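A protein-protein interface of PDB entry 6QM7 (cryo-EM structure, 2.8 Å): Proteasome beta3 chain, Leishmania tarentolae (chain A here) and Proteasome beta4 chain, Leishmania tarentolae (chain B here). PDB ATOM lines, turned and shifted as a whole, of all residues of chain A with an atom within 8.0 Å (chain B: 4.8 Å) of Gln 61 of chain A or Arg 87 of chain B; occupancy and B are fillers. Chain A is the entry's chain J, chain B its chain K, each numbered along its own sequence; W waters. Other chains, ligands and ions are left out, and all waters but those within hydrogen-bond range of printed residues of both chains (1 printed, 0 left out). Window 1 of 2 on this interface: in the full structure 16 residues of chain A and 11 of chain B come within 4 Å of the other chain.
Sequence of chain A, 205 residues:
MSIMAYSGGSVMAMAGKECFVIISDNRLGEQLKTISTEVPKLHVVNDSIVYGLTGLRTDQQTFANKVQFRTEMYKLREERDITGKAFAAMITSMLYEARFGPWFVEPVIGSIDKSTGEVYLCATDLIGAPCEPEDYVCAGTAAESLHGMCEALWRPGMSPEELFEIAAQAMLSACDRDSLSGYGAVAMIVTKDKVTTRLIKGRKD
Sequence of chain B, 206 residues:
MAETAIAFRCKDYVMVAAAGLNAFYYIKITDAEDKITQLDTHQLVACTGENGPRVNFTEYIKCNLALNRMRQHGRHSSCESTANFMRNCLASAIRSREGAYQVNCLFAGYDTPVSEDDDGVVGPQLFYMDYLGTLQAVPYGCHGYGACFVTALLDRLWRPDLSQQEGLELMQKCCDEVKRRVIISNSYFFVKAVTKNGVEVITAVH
O of Thr 58 of chain A lies within hydrogen-bond range of NH2 of Arg 87 of chain B. The side-chain hydroxyl (OG1) of Thr 62 of chain A sits at hydrogen-bond distance from the guanidinium group (NH2) of Arg 87 of chain B (2.6 Å). OE1 of Gln 61 of chain A is in hydrogen-bond range of N of Leu 135 of chain B (2.7 Å).
O of Thr 58 of chain A sits at hydrogen-bond distance from OG1 of Thr 62 of chain A, at 3.1 Å. The backbone carbonyl oxygen (O) of Gly 133 of chain B is in hydrogen-bond range of the guanidinium group (NE) of Arg 87 of chain B (2.5 Å). The side-chain amide oxygen (OE1) of Gln 60 of chain A is in hydrogen-bond range of the guanidinium group (NH1) of Arg 57 of chain A (2.7 Å). O of Gln 61 of chain A lies close to ND2 of Asn 65 of chain A, 3.3 Å away.
Among the printed residues, pairs that only touch across the chains: Gln 61 of chain A with Thr 134 of chain B (3.4 Å), Thr 62 of chain A with Ala 91 of chain B (3.6 Å), Gln 61 of chain A with Arg 87 of chain B (3.7 Å), Gln 61 of chain A with Gly 133 of chain B (3.7 Å), Arg 57 of chain A with Thr 134 of chain B (3.7 Å), Thr 58 of chain A with Gly 133 of chain B (3.7 Å), Thr 58 of chain A with Thr 134 of chain B (3.7 Å), Asn 65 of chain A with Arg 87 of chain B (3.8 Å) and Thr 58 of chain A with Ala 91 of chain B (3.8 Å).
Of chain B, only Arg 87 (3.7 Å), Gly 133 (3.7 Å), Thr 134 (3.4 Å) and Leu 135 (2.7 Å) come within 4 Å of Gln 61 of chain A. Printed residues of chain B within 4 Å of Thr 62 of chain A: Arg 87 and Ala 91. Of the printed residues of chain B, Asn 65 of chain A touches Arg 87. Met 86 of chain B touches none of the printed residues of chain A. Printed residues of chain A within 4 Å of Arg 87 of chain B: Thr 58 (2.9 Å), Gln 61 (3.7 Å), Thr 62 (2.6 Å) and Asn 65 (3.8 Å). Cys 89 of chain B touches none of the printed residues of chain A. Of the printed residues of chain A, Ala 91 of chain B touches Thr 58 and Thr 62. Of the printed residues of chain A, Gly 133 of chain B touches Thr 58 (3.7 Å) and Gln 61 (3.7 Å). Of the printed residues of chain A, Leu 135 of chain B touches Gln 61 (2.7 Å). The nearest printed residue of chain A that does not touch Ala 91 of chain B is Asp 59 of chain A (6.3 Å).
Of the 23 printed residues of chain A, 5 touch a printed residue of chain B. Printed residues of chain A that touch a printed residue of chain B: Arg 57, Thr 58, Gln 61, Thr 62 and Asn 65. Among the printed residues, 12 pairs touch across the chains.
Water W1 lies within hydrogen-bond range of OG1 of Thr 134 of chain B (2.7 Å) and OG1 of Thr 58 of chain A (3.0 Å).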
ATOM      1  N   LEU A  28     -20.180  12.997  28.364  1.00  0.00           N
ATOM      2  CA  LEU A  28     -18.901  13.092  27.621  1.00  0.00           C
ATOM      3  C   LEU A  28     -18.012  11.951  28.104  1.00  0.00           C
ATOM      4  O   LEU A  28     -17.836  11.837  29.314  1.00  0.00           O
ATOM      5  CB  LEU A  28     -18.235  14.442  27.896  1.00  0.00           C
ATOM      6  CG  LEU A  28     -16.807  14.550  27.364  1.00  0.00           C
ATOM      7  CD1 LEU A  28     -16.820  14.558  25.843  1.00  0.00           C
ATOM      8  CD2 LEU A  28     -16.073  15.769  27.907  1.00  0.00           C
ATOM      9  N   VAL A  39     -22.420  17.775  29.942  1.00  0.00           N
ATOM     10  CA  VAL A  39     -21.867  18.252  28.648  1.00  0.00           C
ATOM     11  C   VAL A  39     -22.950  18.094  27.606  1.00  0.00           C
ATOM     12  O   VAL A  39     -22.934  17.131  26.853  1.00  0.00           O
ATOM     13  CB  VAL A  39     -20.601  17.477  28.246  1.00  0.00           C
ATOM     14  CG1 VAL A  39     -19.964  18.027  26.962  1.00  0.00           C
ATOM     15  CG2 VAL A  39     -19.597  17.476  29.386  1.00  0.00           C
ATOM     16  N   HIS A  43     -25.878  24.027  20.622  1.00  0.00           N
ATOM     17  CA  HIS A  43     -25.297  25.373  20.388  1.00  0.00           C
ATOM     18  C   HIS A  43     -26.379  26.261  19.771  1.00  0.00           C
ATOM     19  O   HIS A  43     -27.093  25.800  18.871  1.00  0.00           O
ATOM     20  CB  HIS A  43     -24.066  25.270  19.489  1.00  0.00           C
ATOM     21  CG  HIS A  43     -23.021  24.347  20.006  1.00  0.00           C
ATOM     22  ND1 HIS A  43     -22.083  24.742  20.946  1.00  0.00           N
ATOM     23  CD2 HIS A  43     -22.767  23.049  19.724  1.00  0.00           C
ATOM     24  CE1 HIS A  43     -21.296  23.719  21.226  1.00  0.00           C
ATOM     25  NE2 HIS A  43     -21.697  22.663  20.485  1.00  0.00           N
ATOM     26  N   TYR A  51     -28.198  24.079  16.797  1.00  0.00           N
ATOM     27  CA  TYR A  51     -27.566  22.875  16.223  1.00  0.00           C
ATOM     28  C   TYR A  51     -26.918  22.071  17.337  1.00  0.00           C
ATOM     29  O   TYR A  51     -26.657  22.605  18.397  1.00  0.00           O
ATOM     30  CB  TYR A  51     -26.626  23.241  15.079  1.00  0.00           C
ATOM     31  CG  TYR A  51     -25.301  23.856  15.443  1.00  0.00           C
ATOM     32  CD1 TYR A  51     -24.121  23.147  15.305  1.00  0.00           C
ATOM     33  CD2 TYR A  51     -25.215  25.172  15.836  1.00  0.00           C
ATOM     34  CE1 TYR A  51     -22.892  23.716  15.592  1.00  0.00           C
ATOM     35  CE2 TYR A  51     -23.996  25.764  16.118  1.00  0.00           C
ATOM     36  CZ  TYR A  51     -22.824  25.031  16.013  1.00  0.00           C
ATOM     37  OH  TYR A  51     -21.615  25.608  16.300  1.00  0.00           O
ATOM     38  N   LEU A  53     -23.755  19.022  17.789  1.00  0.00           N
ATOM     39  CA  LEU A  53     -22.650  18.302  17.133  1.00  0.00           C
ATOM     40  C   LEU A  53     -22.426  17.016  17.899  1.00  0.00           C
ATOM     41  O   LEU A  53     -22.252  17.072  19.112  1.00  0.00           O
ATOM     42  CB  LEU A  53     -21.403  19.175  17.167  1.00  0.00           C
ATOM     43  CG  LEU A  53     -21.439  20.392  16.253  1.00  0.00           C
ATOM     44  CD1 LEU A  53     -20.291  21.318  16.598  1.00  0.00           C
ATOM     45  CD2 LEU A  53     -21.346  19.986  14.793  1.00  0.00           C
ATOM     46  N   THR A  54     -22.461  15.901  17.210  1.00  0.00           N
ATOM     47  CA  THR A  54     -22.009  14.610  17.757  1.00  0.00           C
ATOM     48  C   THR A  54     -20.597  14.411  17.232  1.00  0.00           C
ATOM     49  O   THR A  54     -20.104  15.307  16.546  1.00  0.00           O
ATOM     50  CB  THR A  54     -23.007  13.517  17.370  1.00  0.00           C
ATOM     51  OG1 THR A  54     -23.237  13.623  15.962  1.00  0.00           O
ATOM     52  CG2 THR A  54     -24.305  13.677  18.127  1.00  0.00           C
ATOM     53  N   GLY A  55     -20.002  13.270  17.523  1.00  0.00           N
ATOM     54  CA  GLY A  55     -18.691  12.901  16.988  1.00  0.00           C
ATOM     55  C   GLY A  55     -17.617  13.205  17.991  1.00  0.00           C
ATOM     56  O   GLY A  55     -17.956  13.401  19.161  1.00  0.00           O
ATOM     57  N   LEU A  56     -16.373  13.220  17.529  1.00  0.00           N
ATOM     58  CA  LEU A  56     -15.181  13.300  18.396  1.00  0.00           C
ATOM     59  C   LEU A  56     -15.208  14.650  19.099  1.00  0.00           C
ATOM     60  O   LEU A  56     -15.344  15.648  18.394  1.00  0.00           O
ATOM     61  CB  LEU A  56     -13.942  13.131  17.516  1.00  0.00           C
ATOM     62  CG  LEU A  56     -12.622  13.106  18.274  1.00  0.00           C
ATOM     63  CD1 LEU A  56     -12.587  11.925  19.232  1.00  0.00           C
ATOM     64  CD2 LEU A  56     -11.456  13.079  17.302  1.00  0.00           C
ATOM     65  N   ARG A  57     -15.082  14.671  20.424  1.00  0.00           N
ATOM     66  CA  ARG A  57     -15.413  15.879  21.229  1.00  0.00           C
ATOM     67  C   ARG A  57     -14.522  17.051  20.825  1.00  0.00           C
ATOM     68  O   ARG A  57     -15.050  18.165  20.732  1.00  0.00           O
ATOM     69  CB  ARG A  57     -15.250  15.652  22.735  1.00  0.00           C
ATOM     70  CG  ARG A  57     -15.562  16.863  23.600  1.00  0.00           C
ATOM     71  CD  ARG A  57     -16.963  17.356  23.343  1.00  0.00           C
ATOM     72  NE  ARG A  57     -17.234  18.566  24.089  1.00  0.00           N
ATOM     73  CZ  ARG A  57     -18.298  19.331  23.912  1.00  0.00           C
ATOM     74  NH1 ARG A  57     -19.212  19.029  23.006  1.00  0.00           N
ATOM     75  NH2 ARG A  57     -18.445  20.412  24.648  1.00  0.00           N
ATOM     76  N   THR A  58     -13.222  16.804  20.651  1.00  0.00           N
ATOM     77  CA  THR A  58     -12.263  17.760  20.046  1.00  0.00           C
ATOM     78  C   THR A  58     -12.881  18.475  18.848  1.00  0.00           C
ATOM     79  O   THR A  58     -12.772  19.687  18.775  1.00  0.00           O
ATOM     80  CB  THR A  58     -11.066  17.080  19.384  1.00  0.00           C
ATOM     81  OG1 THR A  58     -10.823  15.799  19.954  1.00  0.00           O
ATOM     82  CG2 THR A  58      -9.858  17.976  19.471  1.00  0.00           C
ATOM     83  N   ASP A  59     -13.448  17.711  17.917  1.00  0.00           N
ATOM     84  CA  ASP A  59     -13.926  18.239  16.621  1.00  0.00           C
ATOM     85  C   ASP A  59     -15.257  18.939  16.853  1.00  0.00           C
ATOM     86  O   ASP A  59     -15.471  19.976  16.238  1.00  0.00           O
ATOM     87  CB  ASP A  59     -13.990  17.146  15.558  1.00  0.00           C
ATOM     88  CG  ASP A  59     -12.627  16.671  15.086  1.00  0.00           C
ATOM     89  OD1 ASP A  59     -12.578  15.923  14.089  1.00  0.00           O
ATOM     90  OD2 ASP A  59     -11.610  17.069  15.710  1.00  0.00           O
ATOM     91  N   GLN A  60     -16.105  18.416  17.724  1.00  0.00           N
ATOM     92  CA  GLN A  60     -17.313  19.158  18.136  1.00  0.00           C
ATOM     93  C   GLN A  60     -16.873  20.536  18.621  1.00  0.00           C
ATOM     94  O   GLN A  60     -17.514  21.506  18.242  1.00  0.00           O
ATOM     95  CB  GLN A  60     -18.076  18.509  19.287  1.00  0.00           C
ATOM     96  CG  GLN A  60     -18.421  17.051  19.082  1.00  0.00           C
ATOM     97  CD  GLN A  60     -19.183  16.537  20.266  1.00  0.00           C
ATOM     98  OE1 GLN A  60     -19.811  17.301  20.993  1.00  0.00           O
ATOM     99  NE2 GLN A  60     -19.132  15.233  20.454  1.00  0.00           N
ATOM    100  N   GLN A  61     -15.819  20.617  19.428  1.00  0.00           N
ATOM    101  CA  GLN A  61     -15.394  21.897  20.045  1.00  0.00           C
ATOM    102  C   GLN A  61     -14.714  22.784  19.012  1.00  0.00           C
ATOM    103  O   GLN A  61     -15.015  23.985  19.015  1.00  0.00           O
ATOM    104  CB  GLN A  61     -14.479  21.669  21.238  1.00  0.00           C
ATOM    105  CG  GLN A  61     -15.232  21.066  22.405  1.00  0.00           C
ATOM    106  CD  GLN A  61     -14.378  21.017  23.638  1.00  0.00           C
ATOM    107  OE1 GLN A  61     -13.394  20.283  23.697  1.00  0.00           O
ATOM    108  NE2 GLN A  61     -14.768  21.793  24.635  1.00  0.00           N
ATOM    109  N   THR A  62     -13.825  22.224  18.197  1.00  0.00           N
ATOM    110  CA  THR A  62     -13.118  22.975  17.133  1.00  0.00           C
ATOM    111  C   THR A  62     -14.150  23.421  16.108  1.00  0.00           C
ATOM    112  O   THR A  62     -14.229  24.619  15.850  1.00  0.00           O
ATOM    113  CB  THR A  62     -12.012  22.188  16.423  1.00  0.00           C
ATOM    114  OG1 THR A  62     -11.008  21.747  17.332  1.00  0.00           O
ATOM    115  CG2 THR A  62     -11.303  23.032  15.388  1.00  0.00           C
ATOM    116  N   PHE A  63     -14.920  22.495  15.561  1.00  0.00           N
ATOM    117  CA  PHE A  63     -15.950  22.805  14.541  1.00  0.00           C
ATOM    118  C   PHE A  63     -16.924  23.848  15.088  1.00  0.00           C
ATOM    119  O   PHE A  63     -17.205  24.788  14.359  1.00  0.00           O
ATOM    120  CB  PHE A  63     -16.711  21.561  14.092  1.00  0.00           C
ATOM    121  CG  PHE A  63     -17.502  21.809  12.844  1.00  0.00           C
ATOM    122  CD1 PHE A  63     -16.856  21.910  11.619  1.00  0.00           C
ATOM    123  CD2 PHE A  63     -18.866  22.026  12.905  1.00  0.00           C
ATOM    124  CE1 PHE A  63     -17.575  22.166  10.463  1.00  0.00           C
ATOM    125  CE2 PHE A  63     -19.584  22.277  11.748  1.00  0.00           C
ATOM    126  CZ  PHE A  63     -18.937  22.353  10.532  1.00  0.00           C
ATOM    127  N   ALA A  64     -17.407  23.695  16.320  1.00  0.00           N
ATOM    128  CA  ALA A  64     -18.364  24.640  16.940  1.00  0.00           C
ATOM    129  C   ALA A  64     -17.747  26.035  16.992  1.00  0.00           C
ATOM    130  O   ALA A  64     -18.501  27.012  16.782  1.00  0.00           O
ATOM    131  CB  ALA A  64     -18.774  24.208  18.324  1.00  0.00           C
ATOM    132  N   ASN A  65     -16.452  26.131  17.303  1.00  0.00           N
ATOM    133  CA  ASN A  65     -15.726  27.422  17.347  1.00  0.00           C
ATOM    134  C   ASN A  65     -15.697  28.014  15.945  1.00  0.00           C
ATOM    135  O   ASN A  65     -15.913  29.219  15.824  1.00  0.00           O
ATOM    136  CB  ASN A  65     -14.264  27.299  17.781  1.00  0.00           C
ATOM    137  CG  ASN A  65     -14.039  27.078  19.256  1.00  0.00           C
ATOM    138  OD1 ASN A  65     -12.890  26.922  19.669  1.00  0.00           O
ATOM    139  ND2 ASN A  65     -15.107  27.071  20.039  1.00  0.00           N
ATOM    140  N   LYS A  66     -15.316  27.202  14.959  1.00  0.00           N
ATOM    141  CA  LYS A  66     -15.196  27.615  13.542  1.00  0.00           C
ATOM    142  C   LYS A  66     -16.537  28.151  13.080  1.00  0.00           C
ATOM    143  O   LYS A  66     -16.534  29.134  12.374  1.00  0.00           O
ATOM    144  CB  LYS A  66     -14.854  26.449  12.623  1.00  0.00           C
ATOM    145  CG  LYS A  66     -13.395  26.037  12.588  1.00  0.00           C
ATOM    146  CD  LYS A  66     -13.086  25.159  11.380  1.00  0.00           C
ATOM    147  CE  LYS A  66     -11.820  25.577  10.667  1.00  0.00           C
ATOM    148  NZ  LYS A  66     -10.678  25.710  11.614  1.00  0.00           N
ATOM    149  N   VAL A  67     -17.624  27.496  13.468  1.00  0.00           N
ATOM    150  CA  VAL A  67     -19.005  27.903  13.097  1.00  0.00           C
ATOM    151  C   VAL A  67     -19.326  29.215  13.802  1.00  0.00           C
ATOM    152  O   VAL A  67     -19.929  30.069  13.157  1.00  0.00           O
ATOM    153  CB  VAL A  67     -20.032  26.811  13.444  1.00  0.00           C
ATOM    154  CG1 VAL A  67     -21.460  27.339  13.445  1.00  0.00           C
ATOM    155  CG2 VAL A  67     -19.897  25.625  12.502  1.00  0.00           C
ATOM    156  N   GLN A  68     -18.984  29.333  15.081  1.00  0.00           N
ATOM    157  CA  GLN A  68     -19.272  30.543  15.886  1.00  0.00           C
ATOM    158  C   GLN A  68     -18.534  31.736  15.276  1.00  0.00           C
ATOM    159  O   GLN A  68     -19.076  32.841  15.319  1.00  0.00           O
ATOM    160  CB  GLN A  68     -18.865  30.328  17.341  1.00  0.00           C
ATOM    161  CG  GLN A  68     -19.345  31.409  18.304  1.00  0.00           C
ATOM    162  CD  GLN A  68     -18.424  31.491  19.497  1.00  0.00           C
ATOM    163  OE1 GLN A  68     -18.326  30.553  20.290  1.00  0.00           O
ATOM    164  NE2 GLN A  68     -17.709  32.601  19.614  1.00  0.00           N
ATOM    165  N   TRP A 103     -13.625  16.517   9.522  1.00  0.00           N
ATOM    166  CA  TRP A 103     -14.029  16.756  10.925  1.00  0.00           C
ATOM    167  C   TRP A 103     -14.879  15.573  11.340  1.00  0.00           C
ATOM    168  O   TRP A 103     -15.854  15.321  10.648  1.00  0.00           O
ATOM    169  CB  TRP A 103     -14.842  18.046  11.070  1.00  0.00           C
ATOM    170  CG  TRP A 103     -14.104  19.268  10.636  1.00  0.00           C
ATOM    171  CD1 TRP A 103     -14.301  19.998   9.505  1.00  0.00           C
ATOM    172  CD2 TRP A 103     -13.015  19.880  11.331  1.00  0.00           C
ATOM    173  NE1 TRP A 103     -13.407  21.030   9.450  1.00  0.00           N
ATOM    174  CE2 TRP A 103     -12.606  20.985  10.557  1.00  0.00           C
ATOM    175  CE3 TRP A 103     -12.349  19.598  12.531  1.00  0.00           C
ATOM    176  CZ2 TRP A 103     -11.552  21.807  10.943  1.00  0.00           C
ATOM    177  CZ3 TRP A 103     -11.311  20.411  12.918  1.00  0.00           C
ATOM    178  CH2 TRP A 103     -10.922  21.503  12.133  1.00  0.00           C
ATOM    179  N   PHE A 104     -14.540  14.910  12.435  1.00  0.00           N
ATOM    180  CA  PHE A 104     -15.353  13.819  13.015  1.00  0.00           C
ATOM    181  C   PHE A 104     -16.470  14.457  13.826  1.00  0.00           C
ATOM    182  O   PHE A 104     -16.443  14.406  15.058  1.00  0.00           O
ATOM    183  CB  PHE A 104     -14.458  12.869  13.804  1.00  0.00           C
ATOM    184  CG  PHE A 104     -13.431  12.233  12.912  1.00  0.00           C
ATOM    185  CD1 PHE A 104     -13.820  11.313  11.948  1.00  0.00           C
ATOM    186  CD2 PHE A 104     -12.097  12.616  12.980  1.00  0.00           C
ATOM    187  CE1 PHE A 104     -12.885  10.763  11.085  1.00  0.00           C
ATOM    188  CE2 PHE A 104     -11.161  12.060  12.122  1.00  0.00           C
ATOM    189  CZ  PHE A 104     -11.559  11.136  11.174  1.00  0.00           C
ATOM    190  N   VAL A 105     -17.419  15.053  13.119  1.00  0.00           N
ATOM    191  CA  VAL A 105     -18.657  15.637  13.685  1.00  0.00           C
ATOM    192  C   VAL A 105     -19.803  15.307  12.747  1.00  0.00           C
ATOM    193  O   VAL A 105     -19.573  15.190  11.548  1.00  0.00           O
ATOM    194  CB  VAL A 105     -18.540  17.153  13.870  1.00  0.00           C
ATOM    195  CG1 VAL A 105     -17.353  17.505  14.737  1.00  0.00           C
ATOM    196  CG2 VAL A 105     -18.474  17.895  12.552  1.00  0.00           C
ATOM    197  N   ALA B  83      -7.045  27.925  28.996  1.00  0.00           N
ATOM    198  CA  ALA B  83      -7.584  26.571  28.750  1.00  0.00           C
ATOM    199  C   ALA B  83      -7.933  26.452  27.275  1.00  0.00           C
ATOM    200  O   ALA B  83      -7.575  25.439  26.674  1.00  0.00           O
ATOM    201  CB  ALA B  83      -8.792  26.303  29.612  1.00  0.00           C
ATOM    202  N   ASN B  84      -8.595  27.465  26.719  1.00  0.00           N
ATOM    203  CA  ASN B  84      -9.023  27.485  25.295  1.00  0.00           C
ATOM    204  C   ASN B  84      -7.796  27.645  24.419  1.00  0.00           C
ATOM    205  O   ASN B  84      -7.679  26.907  23.439  1.00  0.00           O
ATOM    206  CB  ASN B  84     -10.112  28.517  25.041  1.00  0.00           C
ATOM    207  CG  ASN B  84     -11.455  27.955  25.445  1.00  0.00           C
ATOM    208  OD1 ASN B  84     -11.893  26.934  24.909  1.00  0.00           O
ATOM    209  ND2 ASN B  84     -12.083  28.562  26.435  1.00  0.00           N
ATOM    210  N   PHE B  85      -6.896  28.540  24.785  1.00  0.00           N
ATOM    211  CA  PHE B  85      -5.613  28.695  24.067  1.00  0.00           C
ATOM    212  C   PHE B  85      -4.898  27.349  23.982  1.00  0.00           C
ATOM    213  O   PHE B  85      -4.394  27.042  22.893  1.00  0.00           O
ATOM    214  CB  PHE B  85      -4.692  29.694  24.757  1.00  0.00           C
ATOM    215  CG  PHE B  85      -3.349  29.782  24.088  1.00  0.00           C
ATOM    216  CD1 PHE B  85      -3.255  30.184  22.767  1.00  0.00           C
ATOM    217  CD2 PHE B  85      -2.189  29.464  24.772  1.00  0.00           C
ATOM    218  CE1 PHE B  85      -2.028  30.278  22.140  1.00  0.00           C
ATOM    219  CE2 PHE B  85      -0.958  29.560  24.141  1.00  0.00           C
ATOM    220  CZ  PHE B  85      -0.881  29.966  22.826  1.00  0.00           C
ATOM    221  N   MET B  86      -4.851  26.608  25.093  1.00  0.00           N
ATOM    222  CA  MET B  86      -4.153  25.302  25.215  1.00  0.00           C
ATOM    223  C   MET B  86      -4.871  24.279  24.349  1.00  0.00           C
ATOM    224  O   MET B  86      -4.178  23.588  23.608  1.00  0.00           O
ATOM    225  CB  MET B  86      -4.113  24.795  26.657  1.00  0.00           C
ATOM    226  CG  MET B  86      -3.201  25.608  27.579  1.00  0.00           C
ATOM    227  SD  MET B  86      -3.290  25.179  29.348  1.00  0.00           S
ATOM    228  CE  MET B  86      -3.092  23.401  29.207  1.00  0.00           C
ATOM    229  N   ARG B  87      -6.204  24.194  24.431  1.00  0.00           N
ATOM    230  CA  ARG B  87      -6.985  23.147  23.701  1.00  0.00           C
ATOM    231  C   ARG B  87      -6.876  23.397  22.198  1.00  0.00           C
ATOM    232  O   ARG B  87      -6.881  22.417  21.449  1.00  0.00           O
ATOM    233  CB  ARG B  87      -8.459  23.071  24.120  1.00  0.00           C
ATOM    234  CG  ARG B  87      -9.429  23.847  23.242  1.00  0.00           C
ATOM    235  CD  ARG B  87     -10.783  23.193  23.105  1.00  0.00           C
ATOM    236  NE  ARG B  87     -10.777  22.222  22.045  1.00  0.00           N
ATOM    237  CZ  ARG B  87     -10.842  22.512  20.761  1.00  0.00           C
ATOM    238  NH1 ARG B  87     -10.910  23.762  20.325  1.00  0.00           N
ATOM    239  NH2 ARG B  87     -10.836  21.519  19.901  1.00  0.00           N
ATOM    240  N   ASN B  88      -6.838  24.665  21.788  1.00  0.00           N
ATOM    241  CA  ASN B  88      -6.770  25.036  20.358  1.00  0.00           C
ATOM    242  C   ASN B  88      -5.394  24.576  19.881  1.00  0.00           C
ATOM    243  O   ASN B  88      -5.294  24.077  18.755  1.00  0.00           O
ATOM    244  CB  ASN B  88      -7.076  26.522  20.126  1.00  0.00           C
ATOM    245  CG  ASN B  88      -6.387  27.062  18.885  1.00  0.00           C
ATOM    246  OD1 ASN B  88      -5.295  27.645  18.966  1.00  0.00           O
ATOM    247  ND2 ASN B  88      -6.996  26.827  17.730  1.00  0.00           N
ATOM    248  N   CYS B  89      -4.382  24.719  20.730  1.00  0.00           N
ATOM    249  CA  CYS B  89      -2.982  24.335  20.428  1.00  0.00           C
ATOM    250  C   CYS B  89      -2.869  22.808  20.273  1.00  0.00           C
ATOM    251  O   CYS B  89      -2.205  22.367  19.321  1.00  0.00           O
ATOM    252  CB  CYS B  89      -2.032  24.891  21.483  1.00  0.00           C
ATOM    253  SG  CYS B  89      -0.470  23.982  21.564  1.00  0.00           S
ATOM    254  N   LEU B  90      -3.499  22.048  21.170  1.00  0.00           N
ATOM    255  CA  LEU B  90      -3.569  20.564  21.142  1.00  0.00           C
ATOM    256  C   LEU B  90      -4.354  20.084  19.931  1.00  0.00           C
ATOM    257  O   LEU B  90      -3.991  19.034  19.375  1.00  0.00           O
ATOM    258  CB  LEU B  90      -4.289  20.057  22.385  1.00  0.00           C
ATOM    259  CG  LEU B  90      -3.526  20.194  23.694  1.00  0.00           C
ATOM    260  CD1 LEU B  90      -4.407  19.795  24.873  1.00  0.00           C
ATOM    261  CD2 LEU B  90      -2.252  19.367  23.669  1.00  0.00           C
ATOM    262  N   ALA B  91      -5.451  20.766  19.626  1.00  0.00           N
ATOM    263  CA  ALA B  91      -6.405  20.381  18.570  1.00  0.00           C
ATOM    264  C   ALA B  91      -5.787  20.684  17.211  1.00  0.00           C
ATOM    265  O   ALA B  91      -5.959  19.872  16.302  1.00  0.00           O
ATOM    266  CB  ALA B  91      -7.724  21.089  18.753  1.00  0.00           C
ATOM    267  N   SER B  92      -5.136  21.831  17.071  1.00  0.00           N
ATOM    268  CA  SER B  92      -4.387  22.211  15.845  1.00  0.00           C
ATOM    269  C   SER B  92      -3.429  21.073  15.505  1.00  0.00           C
ATOM    270  O   SER B  92      -3.431  20.633  14.353  1.00  0.00           O
ATOM    271  CB  SER B  92      -3.649  23.515  16.016  1.00  0.00           C
ATOM    272  OG  SER B  92      -4.555  24.606  16.108  1.00  0.00           O
ATOM    273  N   MET B 129      -8.306  18.152  30.013  1.00  0.00           N
ATOM    274  CA  MET B 129      -7.973  18.231  28.564  1.00  0.00           C
ATOM    275  C   MET B 129      -7.337  16.927  28.116  1.00  0.00           C
ATOM    276  O   MET B 129      -6.338  16.541  28.696  1.00  0.00           O
ATOM    277  CB  MET B 129      -7.046  19.392  28.195  1.00  0.00           C
ATOM    278  CG  MET B 129      -7.127  20.569  29.161  1.00  0.00           C
ATOM    279  SD  MET B 129      -6.611  22.221  28.576  1.00  0.00           S
ATOM    280  CE  MET B 129      -6.060  21.826  26.917  1.00  0.00           C
ATOM    281  N   GLY B 133      -7.424  17.472  22.340  1.00  0.00           N
ATOM    282  CA  GLY B 133      -7.866  18.871  22.463  1.00  0.00           C
ATOM    283  C   GLY B 133      -9.249  18.991  23.065  1.00  0.00           C
ATOM    284  O   GLY B 133      -9.796  20.104  23.062  1.00  0.00           O
ATOM    285  N   THR B 134      -9.816  17.882  23.527  1.00  0.00           N
ATOM    286  CA  THR B 134     -11.054  17.838  24.330  1.00  0.00           C
ATOM    287  C   THR B 134     -10.858  18.719  25.561  1.00  0.00           C
ATOM    288  O   THR B 134     -10.047  18.338  26.386  1.00  0.00           O
ATOM    289  CB  THR B 134     -11.326  16.404  24.788  1.00  0.00           C
ATOM    290  OG1 THR B 134     -11.389  15.558  23.634  1.00  0.00           O
ATOM    291  CG2 THR B 134     -12.574  16.306  25.639  1.00  0.00           C
ATOM    292  N   LEU B 135     -11.540  19.850  25.665  1.00  0.00           N
ATOM    293  CA  LEU B 135     -11.568  20.683  26.893  1.00  0.00           C
ATOM    294  C   LEU B 135     -12.901  20.467  27.604  1.00  0.00           C
ATOM    295  O   LEU B 135     -13.941  20.500  26.929  1.00  0.00           O
ATOM    296  CB  LEU B 135     -11.406  22.145  26.470  1.00  0.00           C
ATOM    297  CG  LEU B 135     -11.338  23.172  27.594  1.00  0.00           C
ATOM    298  CD1 LEU B 135     -10.125  22.905  28.462  1.00  0.00           C
ATOM    299  CD2 LEU B 135     -11.279  24.586  27.031  1.00  0.00           C
HETATM  300  O   HOH W   1     -11.935  13.678  21.831  1.00  0.00           O
